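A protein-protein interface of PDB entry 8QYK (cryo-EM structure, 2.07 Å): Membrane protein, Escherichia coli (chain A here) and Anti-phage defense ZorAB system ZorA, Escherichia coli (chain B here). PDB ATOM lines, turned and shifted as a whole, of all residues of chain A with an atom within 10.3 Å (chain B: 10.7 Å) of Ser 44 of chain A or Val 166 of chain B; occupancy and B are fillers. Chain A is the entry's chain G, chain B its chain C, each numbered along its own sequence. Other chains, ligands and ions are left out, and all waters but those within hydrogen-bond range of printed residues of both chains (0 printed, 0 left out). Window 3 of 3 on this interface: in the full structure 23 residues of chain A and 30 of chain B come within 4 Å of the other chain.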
ATOM      1  N   LEU A  36     -22.028 -12.865  18.337  1.00  0.00           N
ATOM      2  CA  LEU A  36     -23.130 -12.051  18.842  1.00  0.00           C
ATOM      3  C   LEU A  36     -22.938 -10.579  18.498  1.00  0.00           C
ATOM      4  O   LEU A  36     -23.851  -9.917  17.989  1.00  0.00           O
ATOM      5  CB  LEU A  36     -23.251 -12.223  20.354  1.00  0.00           C
ATOM      6  CG  LEU A  36     -24.097 -11.168  21.070  1.00  0.00           C
ATOM      7  CD1 LEU A  36     -25.554 -11.242  20.645  1.00  0.00           C
ATOM      8  CD2 LEU A  36     -23.960 -11.302  22.573  1.00  0.00           C
ATOM      9  N   VAL A  37     -21.748 -10.047  18.778  1.00  0.00           N
ATOM     10  CA  VAL A  37     -21.511  -8.623  18.580  1.00  0.00           C
ATOM     11  C   VAL A  37     -21.458  -8.284  17.098  1.00  0.00           C
ATOM     12  O   VAL A  37     -21.922  -7.214  16.684  1.00  0.00           O
ATOM     13  CB  VAL A  37     -20.235  -8.204  19.331  1.00  0.00           C
ATOM     14  CG1 VAL A  37     -19.856  -6.776  18.995  1.00  0.00           C
ATOM     15  CG2 VAL A  37     -20.454  -8.358  20.823  1.00  0.00           C
ATOM     16  N   VAL A  38     -20.914  -9.178  16.272  1.00  0.00           N
ATOM     17  CA  VAL A  38     -20.924  -8.963  14.831  1.00  0.00           C
ATOM     18  C   VAL A  38     -22.351  -8.956  14.307  1.00  0.00           C
ATOM     19  O   VAL A  38     -22.701  -8.143  13.448  1.00  0.00           O
ATOM     20  CB  VAL A  38     -20.060 -10.022  14.124  1.00  0.00           C
ATOM     21  CG1 VAL A  38     -20.344 -10.038  12.630  1.00  0.00           C
ATOM     22  CG2 VAL A  38     -18.598  -9.749  14.380  1.00  0.00           C
ATOM     23  N   MET A  39     -23.201  -9.850  14.816  1.00  0.00           N
ATOM     24  CA  MET A  39     -24.602  -9.825  14.416  1.00  0.00           C
ATOM     25  C   MET A  39     -25.265  -8.515  14.821  1.00  0.00           C
ATOM     26  O   MET A  39     -26.001  -7.918  14.030  1.00  0.00           O
ATOM     27  CB  MET A  39     -25.349 -11.011  15.022  1.00  0.00           C
ATOM     28  CG  MET A  39     -26.830 -11.027  14.701  1.00  0.00           C
ATOM     29  SD  MET A  39     -27.662 -12.466  15.388  1.00  0.00           S
ATOM     30  CE  MET A  39     -28.128 -11.830  16.989  1.00  0.00           C
ATOM     31  N   VAL A  40     -25.014  -8.054  16.048  1.00  0.00           N
ATOM     32  CA  VAL A  40     -25.612  -6.801  16.508  1.00  0.00           C
ATOM     33  C   VAL A  40     -25.177  -5.648  15.612  1.00  0.00           C
ATOM     34  O   VAL A  40     -26.002  -4.859  15.137  1.00  0.00           O
ATOM     35  CB  VAL A  40     -25.249  -6.539  17.981  1.00  0.00           C
ATOM     36  CG1 VAL A  40     -25.542  -5.093  18.358  1.00  0.00           C
ATOM     37  CG2 VAL A  40     -25.998  -7.494  18.890  1.00  0.00           C
ATOM     38  N   ALA A  41     -23.873  -5.560  15.339  1.00  0.00           N
ATOM     39  CA  ALA A  41     -23.347  -4.489  14.500  1.00  0.00           C
ATOM     40  C   ALA A  41     -23.909  -4.554  13.086  1.00  0.00           C
ATOM     41  O   ALA A  41     -24.310  -3.529  12.520  1.00  0.00           O
ATOM     42  CB  ALA A  41     -21.820  -4.558  14.471  1.00  0.00           C
ATOM     43  N   SER A  42     -23.954  -5.753  12.500  1.00  0.00           N
ATOM     44  CA  SER A  42     -24.437  -5.902  11.133  1.00  0.00           C
ATOM     45  C   SER A  42     -25.915  -5.562  11.024  1.00  0.00           C
ATOM     46  O   SER A  42     -26.332  -4.892  10.075  1.00  0.00           O
ATOM     47  CB  SER A  42     -24.179  -7.327  10.646  1.00  0.00           C
ATOM     48  OG  SER A  42     -22.863  -7.737  10.961  1.00  0.00           O
ATOM     49  N   LEU A  43     -26.722  -6.023  11.982  1.00  0.00           N
ATOM     50  CA  LEU A  43     -28.148  -5.714  11.972  1.00  0.00           C
ATOM     51  C   LEU A  43     -28.392  -4.227  12.176  1.00  0.00           C
ATOM     52  O   LEU A  43     -29.270  -3.644  11.531  1.00  0.00           O
ATOM     53  CB  LEU A  43     -28.866  -6.530  13.046  1.00  0.00           C
ATOM     54  CG  LEU A  43     -29.045  -8.016  12.740  1.00  0.00           C
ATOM     55  CD1 LEU A  43     -29.689  -8.735  13.910  1.00  0.00           C
ATOM     56  CD2 LEU A  43     -29.868  -8.194  11.475  1.00  0.00           C
ATOM     57  N   SER A  44     -27.629  -3.596  13.070  1.00  0.00           N
ATOM     58  CA  SER A  44     -27.740  -2.155  13.250  1.00  0.00           C
ATOM     59  C   SER A  44     -27.362  -1.392  11.992  1.00  0.00           C
ATOM     60  O   SER A  44     -27.988  -0.373  11.688  1.00  0.00           O
ATOM     61  CB  SER A  44     -26.864  -1.705  14.416  1.00  0.00           C
ATOM     62  OG  SER A  44     -27.156  -2.445  15.585  1.00  0.00           O
ATOM     63  N   SER A  45     -26.354  -1.861  11.258  1.00  0.00           N
ATOM     64  CA  SER A  45     -25.934  -1.167  10.047  1.00  0.00           C
ATOM     65  C   SER A  45     -26.917  -1.366   8.896  1.00  0.00           C
ATOM     66  O   SER A  45     -27.211  -0.416   8.164  1.00  0.00           O
ATOM     67  CB  SER A  45     -24.539  -1.631   9.638  1.00  0.00           C
ATOM     68  OG  SER A  45     -23.581  -1.282  10.618  1.00  0.00           O
ATOM     69  N   VAL A  46     -27.430  -2.585   8.707  1.00  0.00           N
ATOM     70  CA  VAL A  46     -28.308  -2.821   7.563  1.00  0.00           C
ATOM     71  C   VAL A  46     -29.662  -2.156   7.772  1.00  0.00           C
ATOM     72  O   VAL A  46     -30.371  -1.866   6.803  1.00  0.00           O
ATOM     73  CB  VAL A  46     -28.466  -4.327   7.278  1.00  0.00           C
ATOM     74  CG1 VAL A  46     -27.140  -4.930   6.850  1.00  0.00           C
ATOM     75  CG2 VAL A  46     -29.041  -5.054   8.478  1.00  0.00           C
ATOM     76  N   THR A  47     -30.046  -1.908   9.020  1.00  0.00           N
ATOM     77  CA  THR A  47     -31.318  -1.275   9.330  1.00  0.00           C
ATOM     78  C   THR A  47     -31.170   0.162   9.810  1.00  0.00           C
ATOM     79  O   THR A  47     -32.144   0.734  10.305  1.00  0.00           O
ATOM     80  CB  THR A  47     -32.078  -2.093  10.380  1.00  0.00           C
ATOM     81  OG1 THR A  47     -31.409  -1.994  11.643  1.00  0.00           O
ATOM     82  CG2 THR A  47     -32.168  -3.548   9.968  1.00  0.00           C
ATOM     83  N   GLN A  48     -29.984   0.764   9.670  1.00  0.00           N
ATOM     84  CA  GLN A  48     -29.797   2.121  10.178  1.00  0.00           C
ATOM     85  C   GLN A  48     -30.652   3.132   9.425  1.00  0.00           C
ATOM     86  O   GLN A  48     -31.178   4.066  10.035  1.00  0.00           O
ATOM     87  CB  GLN A  48     -28.322   2.529  10.125  1.00  0.00           C
ATOM     88  CG  GLN A  48     -27.714   2.619   8.737  1.00  0.00           C
ATOM     89  CD  GLN A  48     -26.250   3.011   8.769  1.00  0.00           C
ATOM     90  OE1 GLN A  48     -25.411   2.280   9.294  1.00  0.00           O
ATOM     91  NE2 GLN A  48     -25.935   4.169   8.204  1.00  0.00           N
ATOM     92  N   ARG A  49     -30.796   2.975   8.106  1.00  0.00           N
ATOM     93  CA  ARG A  49     -31.700   3.844   7.361  1.00  0.00           C
ATOM     94  C   ARG A  49     -33.139   3.644   7.816  1.00  0.00           C
ATOM     95  O   ARG A  49     -33.882   4.616   8.008  1.00  0.00           O
ATOM     96  CB  ARG A  49     -31.564   3.582   5.862  1.00  0.00           C
ATOM     97  CG  ARG A  49     -30.406   4.317   5.204  1.00  0.00           C
ATOM     98  CD  ARG A  49     -29.904   3.576   3.977  1.00  0.00           C
ATOM     99  NE  ARG A  49     -28.553   3.984   3.607  1.00  0.00           N
ATOM    100  CZ  ARG A  49     -27.811   3.376   2.693  1.00  0.00           C
ATOM    101  NH1 ARG A  49     -28.254   2.319   2.034  1.00  0.00           N
ATOM    102  NH2 ARG A  49     -26.592   3.841   2.433  1.00  0.00           N
ATOM    103  N   ILE A  50     -33.543   2.388   8.012  1.00  0.00           N
ATOM    104  CA  ILE A  50     -34.877   2.101   8.523  1.00  0.00           C
ATOM    105  C   ILE A  50     -35.051   2.674   9.922  1.00  0.00           C
ATOM    106  O   ILE A  50     -36.107   3.222  10.253  1.00  0.00           O
ATOM    107  CB  ILE A  50     -35.146   0.586   8.492  1.00  0.00           C
ATOM    108  CG1 ILE A  50     -35.017   0.052   7.065  1.00  0.00           C
ATOM    109  CG2 ILE A  50     -36.515   0.269   9.072  1.00  0.00           C
ATOM    110  CD1 ILE A  50     -35.295  -1.421   6.945  1.00  0.00           C
ATOM    111  N   GLN A  51     -34.025   2.551  10.770  1.00  0.00           N
ATOM    112  CA  GLN A  51     -34.124   3.085  12.125  1.00  0.00           C
ATOM    113  C   GLN A  51     -34.245   4.604  12.121  1.00  0.00           C
ATOM    114  O   GLN A  51     -35.027   5.167  12.891  1.00  0.00           O
ATOM    115  CB  GLN A  51     -32.925   2.643  12.965  1.00  0.00           C
ATOM    116  CG  GLN A  51     -32.909   1.158  13.285  1.00  0.00           C
ATOM    117  CD  GLN A  51     -31.611   0.709  13.922  1.00  0.00           C
ATOM    118  OE1 GLN A  51     -30.658   1.481  14.031  1.00  0.00           O
ATOM    119  NE2 GLN A  51     -31.565  -0.548  14.348  1.00  0.00           N
ATOM    120  N   ARG A  52     -33.477   5.285  11.268  1.00  0.00           N
ATOM    121  CA  ARG A  52     -33.594   6.739  11.184  1.00  0.00           C
ATOM    122  C   ARG A  52     -34.961   7.156  10.660  1.00  0.00           C
ATOM    123  O   ARG A  52     -35.559   8.112  11.167  1.00  0.00           O
ATOM    124  CB  ARG A  52     -32.490   7.323  10.304  1.00  0.00           C
ATOM    125  CG  ARG A  52     -31.124   7.366  10.958  1.00  0.00           C
ATOM    126  CD  ARG A  52     -30.200   8.324  10.224  1.00  0.00           C
ATOM    127  NE  ARG A  52     -29.916   7.888   8.862  1.00  0.00           N
ATOM    128  CZ  ARG A  52     -28.910   7.093   8.524  1.00  0.00           C
ATOM    129  NH1 ARG A  52     -28.070   6.617   9.430  1.00  0.00           N
ATOM    130  NH2 ARG A  52     -28.739   6.770   7.246  1.00  0.00           N
ATOM    131  N   GLN A  55     -37.423   6.635  13.470  1.00  0.00           N
ATOM    132  CA  GLN A  55     -37.265   7.676  14.480  1.00  0.00           C
ATOM    133  C   GLN A  55     -37.874   8.989  14.011  1.00  0.00           C
ATOM    134  O   GLN A  55     -38.523   9.695  14.792  1.00  0.00           O
ATOM    135  CB  GLN A  55     -35.785   7.859  14.817  1.00  0.00           C
ATOM    136  CG  GLN A  55     -35.516   8.869  15.920  1.00  0.00           C
ATOM    137  CD  GLN A  55     -34.191   9.580  15.748  1.00  0.00           C
ATOM    138  OE1 GLN A  55     -33.507   9.406  14.739  1.00  0.00           O
ATOM    139  NE2 GLN A  55     -33.821  10.389  16.733  1.00  0.00           N
ATOM    140  N   LYS A  58     -41.636   8.620  14.276  1.00  0.00           N
ATOM    141  CA  LYS A  58     -42.053   8.732  15.670  1.00  0.00           C
ATOM    142  C   LYS A  58     -42.005  10.178  16.148  1.00  0.00           C
ATOM    143  O   LYS A  58     -42.907  10.634  16.857  1.00  0.00           O
ATOM    144  CB  LYS A  58     -41.173   7.847  16.552  1.00  0.00           C
ATOM    145  CG  LYS A  58     -41.459   7.967  18.041  1.00  0.00           C
ATOM    146  CD  LYS A  58     -40.809   6.838  18.823  1.00  0.00           C
ATOM    147  CE  LYS A  58     -39.311   6.776  18.565  1.00  0.00           C
ATOM    148  NZ  LYS A  58     -38.799   5.380  18.604  1.00  0.00           N
ATOM    149  N   GLY B 154     -20.250  -3.721  28.257  1.00  0.00           N
ATOM    150  CA  GLY B 154     -20.765  -3.384  26.940  1.00  0.00           C
ATOM    151  C   GLY B 154     -22.267  -3.568  26.817  1.00  0.00           C
ATOM    152  O   GLY B 154     -22.960  -2.727  26.243  1.00  0.00           O
ATOM    153  N   LEU B 155     -22.791  -4.669  27.359  1.00  0.00           N
ATOM    154  CA  LEU B 155     -24.207  -4.984  27.190  1.00  0.00           C
ATOM    155  C   LEU B 155     -25.093  -4.069  28.023  1.00  0.00           C
ATOM    156  O   LEU B 155     -26.148  -3.625  27.555  1.00  0.00           O
ATOM    157  CB  LEU B 155     -24.465  -6.443  27.559  1.00  0.00           C
ATOM    158  CG  LEU B 155     -23.787  -7.510  26.700  1.00  0.00           C
ATOM    159  CD1 LEU B 155     -23.691  -8.830  27.451  1.00  0.00           C
ATOM    160  CD2 LEU B 155     -24.518  -7.685  25.394  1.00  0.00           C
ATOM    161  N   HIS B 157     -24.664  -1.007  29.019  1.00  0.00           N
ATOM    162  CA  HIS B 157     -24.680   0.378  28.577  1.00  0.00           C
ATOM    163  C   HIS B 157     -25.143   0.539  27.136  1.00  0.00           C
ATOM    164  O   HIS B 157     -25.039   1.639  26.585  1.00  0.00           O
ATOM    165  CB  HIS B 157     -23.295   0.999  28.763  1.00  0.00           C
ATOM    166  CG  HIS B 157     -22.875   1.107  30.195  1.00  0.00           C
ATOM    167  ND1 HIS B 157     -23.763   1.395  31.208  1.00  0.00           N
ATOM    168  CD2 HIS B 157     -21.666   0.958  30.785  1.00  0.00           C
ATOM    169  CE1 HIS B 157     -23.119   1.423  32.361  1.00  0.00           C
ATOM    170  NE2 HIS B 157     -21.845   1.160  32.131  1.00  0.00           N
ATOM    171  N   PHE B 158     -25.645  -0.526  26.514  1.00  0.00           N
ATOM    172  CA  PHE B 158     -26.178  -0.422  25.164  1.00  0.00           C
ATOM    173  C   PHE B 158     -27.401   0.486  25.153  1.00  0.00           C
ATOM    174  O   PHE B 158     -28.384   0.230  25.854  1.00  0.00           O
ATOM    175  CB  PHE B 158     -26.539  -1.806  24.629  1.00  0.00           C
ATOM    176  CG  PHE B 158     -26.996  -1.808  23.198  1.00  0.00           C
ATOM    177  CD1 PHE B 158     -26.079  -1.864  22.163  1.00  0.00           C
ATOM    178  CD2 PHE B 158     -28.345  -1.758  22.888  1.00  0.00           C
ATOM    179  CE1 PHE B 158     -26.498  -1.866  20.849  1.00  0.00           C
ATOM    180  CE2 PHE B 158     -28.769  -1.760  21.577  1.00  0.00           C
ATOM    181  CZ  PHE B 158     -27.844  -1.814  20.555  1.00  0.00           C
ATOM    182  N   ASP B 159     -27.336   1.546  24.353  1.00  0.00           N
ATOM    183  CA  ASP B 159     -28.407   2.539  24.266  1.00  0.00           C
ATOM    184  C   ASP B 159     -29.057   2.463  22.892  1.00  0.00           C
ATOM    185  O   ASP B 159     -28.430   2.829  21.883  1.00  0.00           O
ATOM    186  CB  ASP B 159     -27.864   3.943  24.529  1.00  0.00           C
ATOM    187  CG  ASP B 159     -28.949   4.923  24.926  1.00  0.00           C
ATOM    188  OD1 ASP B 159     -30.091   4.791  24.439  1.00  0.00           O
ATOM    189  OD2 ASP B 159     -28.663   5.825  25.741  1.00  0.00           O
ATOM    190  N   PRO B 160     -30.300   1.997  22.796  1.00  0.00           N
ATOM    191  CA  PRO B 160     -30.977   1.898  21.495  1.00  0.00           C
ATOM    192  C   PRO B 160     -31.836   3.097  21.117  1.00  0.00           C
ATOM    193  O   PRO B 160     -32.478   3.054  20.064  1.00  0.00           O
ATOM    194  CB  PRO B 160     -31.858   0.661  21.695  1.00  0.00           C
ATOM    195  CG  PRO B 160     -32.251   0.740  23.139  1.00  0.00           C
ATOM    196  CD  PRO B 160     -31.104   1.402  23.877  1.00  0.00           C
ATOM    197  N   SER B 161     -31.860   4.154  21.933  1.00  0.00           N
ATOM    198  CA  SER B 161     -32.846   5.218  21.753  1.00  0.00           C
ATOM    199  C   SER B 161     -32.639   5.977  20.448  1.00  0.00           C
ATOM    200  O   SER B 161     -33.611   6.307  19.758  1.00  0.00           O
ATOM    201  CB  SER B 161     -32.800   6.176  22.941  1.00  0.00           C
ATOM    202  OG  SER B 161     -31.491   6.675  23.143  1.00  0.00           O
ATOM    203  N   THR B 162     -31.394   6.261  20.092  1.00  0.00           N
ATOM    204  CA  THR B 162     -31.073   7.120  18.964  1.00  0.00           C
ATOM    205  C   THR B 162     -30.143   6.364  18.029  1.00  0.00           C
ATOM    206  O   THR B 162     -29.301   5.584  18.490  1.00  0.00           O
ATOM    207  CB  THR B 162     -30.408   8.423  19.445  1.00  0.00           C
ATOM    208  OG1 THR B 162     -31.297   9.113  20.332  1.00  0.00           O
ATOM    209  CG2 THR B 162     -30.071   9.342  18.287  1.00  0.00           C
ATOM    210  N   PRO B 163     -30.289   6.547  16.711  1.00  0.00           N
ATOM    211  CA  PRO B 163     -29.385   5.856  15.774  1.00  0.00           C
ATOM    212  C   PRO B 163     -27.910   6.100  16.048  1.00  0.00           C
ATOM    213  O   PRO B 163     -27.106   5.164  15.952  1.00  0.00           O
ATOM    214  CB  PRO B 163     -29.815   6.427  14.418  1.00  0.00           C
ATOM    215  CG  PRO B 163     -31.271   6.682  14.584  1.00  0.00           C
ATOM    216  CD  PRO B 163     -31.469   7.103  16.023  1.00  0.00           C
ATOM    217  N   GLU B 164     -27.529   7.328  16.397  1.00  0.00           N
ATOM    218  CA  GLU B 164     -26.144   7.589  16.769  1.00  0.00           C
ATOM    219  C   GLU B 164     -25.799   6.995  18.127  1.00  0.00           C
ATOM    220  O   GLU B 164     -24.661   6.558  18.335  1.00  0.00           O
ATOM    221  CB  GLU B 164     -25.872   9.094  16.757  1.00  0.00           C
ATOM    222  CG  GLU B 164     -25.929   9.717  15.369  1.00  0.00           C
ATOM    223  CD  GLU B 164     -27.341  10.041  14.924  1.00  0.00           C
ATOM    224  OE1 GLU B 164     -28.278   9.838  15.722  1.00  0.00           O
ATOM    225  OE2 GLU B 164     -27.515  10.490  13.771  1.00  0.00           O
ATOM    226  N   GLN B 165     -26.760   6.953  19.052  1.00  0.00           N
ATOM    227  CA  GLN B 165     -26.545   6.222  20.296  1.00  0.00           C
ATOM    228  C   GLN B 165     -26.366   4.735  20.022  1.00  0.00           C
ATOM    229  O   GLN B 165     -25.543   4.071  20.661  1.00  0.00           O
ATOM    230  CB  GLN B 165     -27.707   6.462  21.259  1.00  0.00           C
ATOM    231  CG  GLN B 165     -27.578   7.740  22.076  1.00  0.00           C
ATOM    232  CD  GLN B 165     -26.509   7.652  23.144  1.00  0.00           C
ATOM    233  OE1 GLN B 165     -26.749   7.151  24.241  1.00  0.00           O
ATOM    234  NE2 GLN B 165     -25.317   8.143  22.828  1.00  0.00           N
ATOM    235  N   VAL B 166     -27.125   4.199  19.061  1.00  0.00           N
ATOM    236  CA  VAL B 166     -26.941   2.812  18.647  1.00  0.00           C
ATOM    237  C   VAL B 166     -25.538   2.600  18.097  1.00  0.00           C
ATOM    238  O   VAL B 166     -24.866   1.620  18.435  1.00  0.00           O
ATOM    239  CB  VAL B 166     -28.012   2.415  17.614  1.00  0.00           C
ATOM    240  CG1 VAL B 166     -27.594   1.160  16.862  1.00  0.00           C
ATOM    241  CG2 VAL B 166     -29.351   2.210  18.292  1.00  0.00           C
ATOM    242  N   SER B 167     -25.075   3.513  17.240  1.00  0.00           N
ATOM    243  CA  SER B 167     -23.744   3.375  16.658  1.00  0.00           C
ATOM    244  C   SER B 167     -22.658   3.437  17.726  1.00  0.00           C
ATOM    245  O   SER B 167     -21.700   2.657  17.693  1.00  0.00           O
ATOM    246  CB  SER B 167     -23.520   4.454  15.600  1.00  0.00           C
ATOM    247  OG  SER B 167     -24.395   4.281  14.501  1.00  0.00           O
ATOM    248  N   SER B 168     -22.784   4.366  18.678  1.00  0.00           N
ATOM    249  CA  SER B 168     -21.798   4.455  19.749  1.00  0.00           C
ATOM    250  C   SER B 168     -21.812   3.203  20.620  1.00  0.00           C
ATOM    251  O   SER B 168     -20.752   2.702  21.007  1.00  0.00           O
ATOM    252  CB  SER B 168     -22.042   5.707  20.593  1.00  0.00           C
ATOM    253  OG  SER B 168     -23.158   5.546  21.446  1.00  0.00           O
ATOM    254  N   SER B 169     -23.002   2.683  20.930  1.00  0.00           N
ATOM    255  CA  SER B 169     -23.092   1.446  21.697  1.00  0.00           C
ATOM    256  C   SER B 169     -22.450   0.284  20.951  1.00  0.00           C
ATOM    257  O   SER B 169     -21.763  -0.547  21.553  1.00  0.00           O
ATOM    258  CB  SER B 169     -24.552   1.135  22.015  1.00  0.00           C
ATOM    259  OG  SER B 169     -25.125   2.126  22.843  1.00  0.00           O
ATOM    260  N   VAL B 170     -22.666   0.208  19.638  1.00  0.00           N
ATOM    261  CA  VAL B 170     -22.074  -0.859  18.835  1.00  0.00           C
ATOM    262  C   VAL B 170     -20.554  -0.742  18.821  1.00  0.00           C
ATOM    263  O   VAL B 170     -19.838  -1.743  18.956  1.00  0.00           O
ATOM    264  CB  VAL B 170     -22.663  -0.834  17.413  1.00  0.00           C
ATOM    265  CG1 VAL B 170     -21.769  -1.585  16.448  1.00  0.00           C
ATOM    266  CG2 VAL B 170     -24.067  -1.418  17.409  1.00  0.00           C
ATOM    267  N   ASN B 171     -20.039   0.478  18.657  1.00  0.00           N
ATOM    268  CA  ASN B 171     -18.595   0.681  18.697  1.00  0.00           C
ATOM    269  C   ASN B 171     -18.021   0.287  20.050  1.00  0.00           C
ATOM    270  O   ASN B 171     -16.967  -0.354  20.121  1.00  0.00           O
ATOM    271  CB  ASN B 171     -18.260   2.136  18.374  1.00  0.00           C
ATOM    272  CG  ASN B 171     -18.537   2.488  16.930  1.00  0.00           C
ATOM    273  OD1 ASN B 171     -18.259   1.705  16.024  1.00  0.00           O
ATOM    274  ND2 ASN B 171     -19.093   3.672  16.708  1.00  0.00           N
ATOM    275  N   ASN B 172     -18.707   0.656  21.134  1.00  0.00           N
ATOM    276  CA  ASN B 172     -18.248   0.282  22.468  1.00  0.00           C
ATOM    277  C   ASN B 172     -18.252  -1.229  22.651  1.00  0.00           C
ATOM    278  O   ASN B 172     -17.325  -1.789  23.244  1.00  0.00           O
ATOM    279  CB  ASN B 172     -19.118   0.951  23.530  1.00  0.00           C
ATOM    280  CG  ASN B 172     -18.965   2.457  23.546  1.00  0.00           C
ATOM    281  OD1 ASN B 172     -17.949   2.995  23.111  1.00  0.00           O
ATOM    282  ND2 ASN B 172     -19.980   3.146  24.046  1.00  0.00           N
ATOM    283  N   LEU B 173     -19.289  -1.907  22.153  1.00  0.00           N
ATOM    284  CA  LEU B 173     -19.340  -3.362  22.250  1.00  0.00           C
ATOM    285  C   LEU B 173     -18.190  -4.006  21.487  1.00  0.00           C
ATOM    286  O   LEU B 173     -17.554  -4.943  21.980  1.00  0.00           O
ATOM    287  CB  LEU B 173     -20.681  -3.875  21.727  1.00  0.00           C
ATOM    288  CG  LEU B 173     -21.776  -4.173  22.751  1.00  0.00           C
ATOM    289  CD1 LEU B 173     -23.038  -4.630  22.042  1.00  0.00           C
ATOM    290  CD2 LEU B 173     -21.316  -5.214  23.762  1.00  0.00           C
ATOM    291  N   LEU B 174     -17.907  -3.513  20.279  1.00  0.00           N
ATOM    292  CA  LEU B 174     -16.782  -4.035  19.508  1.00  0.00           C
ATOM    293  C   LEU B 174     -15.465  -3.803  20.236  1.00  0.00           C
ATOM    294  O   LEU B 174     -14.602  -4.692  20.290  1.00  0.00           O
ATOM    295  CB  LEU B 174     -16.754  -3.385  18.125  1.00  0.00           C
ATOM    296  CG  LEU B 174     -17.846  -3.819  17.149  1.00  0.00           C
ATOM    297  CD1 LEU B 174     -17.931  -2.865  15.971  1.00  0.00           C
ATOM    298  CD2 LEU B 174     -17.587  -5.232  16.673  1.00  0.00           C
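O of Asp 159 of chain B sits at hydrogen-bond distance from N of Val 166 of chain B.
The side-chain amide nitrogen of Gln 48 of chain A sits close to the guanidinium group of Arg 52 of chain A, 3.5 Å away.
The backbone carbonyl oxygen of Ala 41 of chain A is in hydrogen-bond range of the side-chain hydroxyl of Ser 45 of chain A, at 3.0 Å.
The backbone carbonyl oxygen of Pro 163 of chain B is in hydrogen-bond range of the side-chain hydroxyl of Ser 167 of chain B.
The side-chain hydroxyl (OG) of Ser 44 of chain A lies within hydrogen-bond range of the backbone carbonyl oxygen (O) of Val 40 of chain A, 2.7 Å away.
Val 37 of chain A touches Leu 174 of chain B (CG1 to CD2, 3.6 Å).
Val 170 of chain B touches Ala 41 of chain A.
Val 166 of chain B touches Ser 44 of chain A (CG1 to CB, 3.8 Å).
Val 170 of chain B touches Ser 44 of chain A (CG2 to OG, 3.7 Å).
Arg 52 of chain A touches Pro 163 of chain B.
CD of Pro 163 of chain B touches OE1 of Gln 55 of chain A, 3.3 Å away.
Of chain B, only Val 166 and Val 170 come within 4 Å of Ser 44 of chain A.
Val 166 of chain B touches just one residue of chain A: Ser 44.
No residue of chain B comes within 4 Å of Leu 43 of chain A.
No residue of chain B comes within 4 Å of Ser 45 of chain A.
Val 46 of chain A touches none of the printed residues of chain B.
Gln 48 of chain A touches none of the printed residues of chain B.
Ser 168 of chain B touches none of the printed residues of chain A.
No residue of chain A comes within 4 Å of Ser 169 of chain B.
Val 170 of chain B touches just these residues of chain A: Ala 41 (3.6 Å) and Ser 44 (3.7 Å).
Of the printed residues of chain A, Leu 174 of chain B touches Val 37 (3.6 Å).
Printed residues of chain B within 4 Å of Arg 52 of chain A: Pro 163.
Of the printed residues of chain B, Val 37 of chain A touches Leu 174 (3.6 Å).
Printed residues of chain B within 4 Å of Gln 55 of chain A: Pro 163 (3.3 Å).
Leu 155 of chain B touches none of the printed residues of chain A.
The nearest residue of chain B that does not touch Ser 44 of chain A is Phe 158 of chain B (5.1 Å).
Hydrophobic or aromatic side chains of chain B that line the printed part of chain A: Pro 163, Val 166, Val 170 and Leu 174.
Of the 19 printed residues of chain A, 5 touch a printed residue of chain B.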
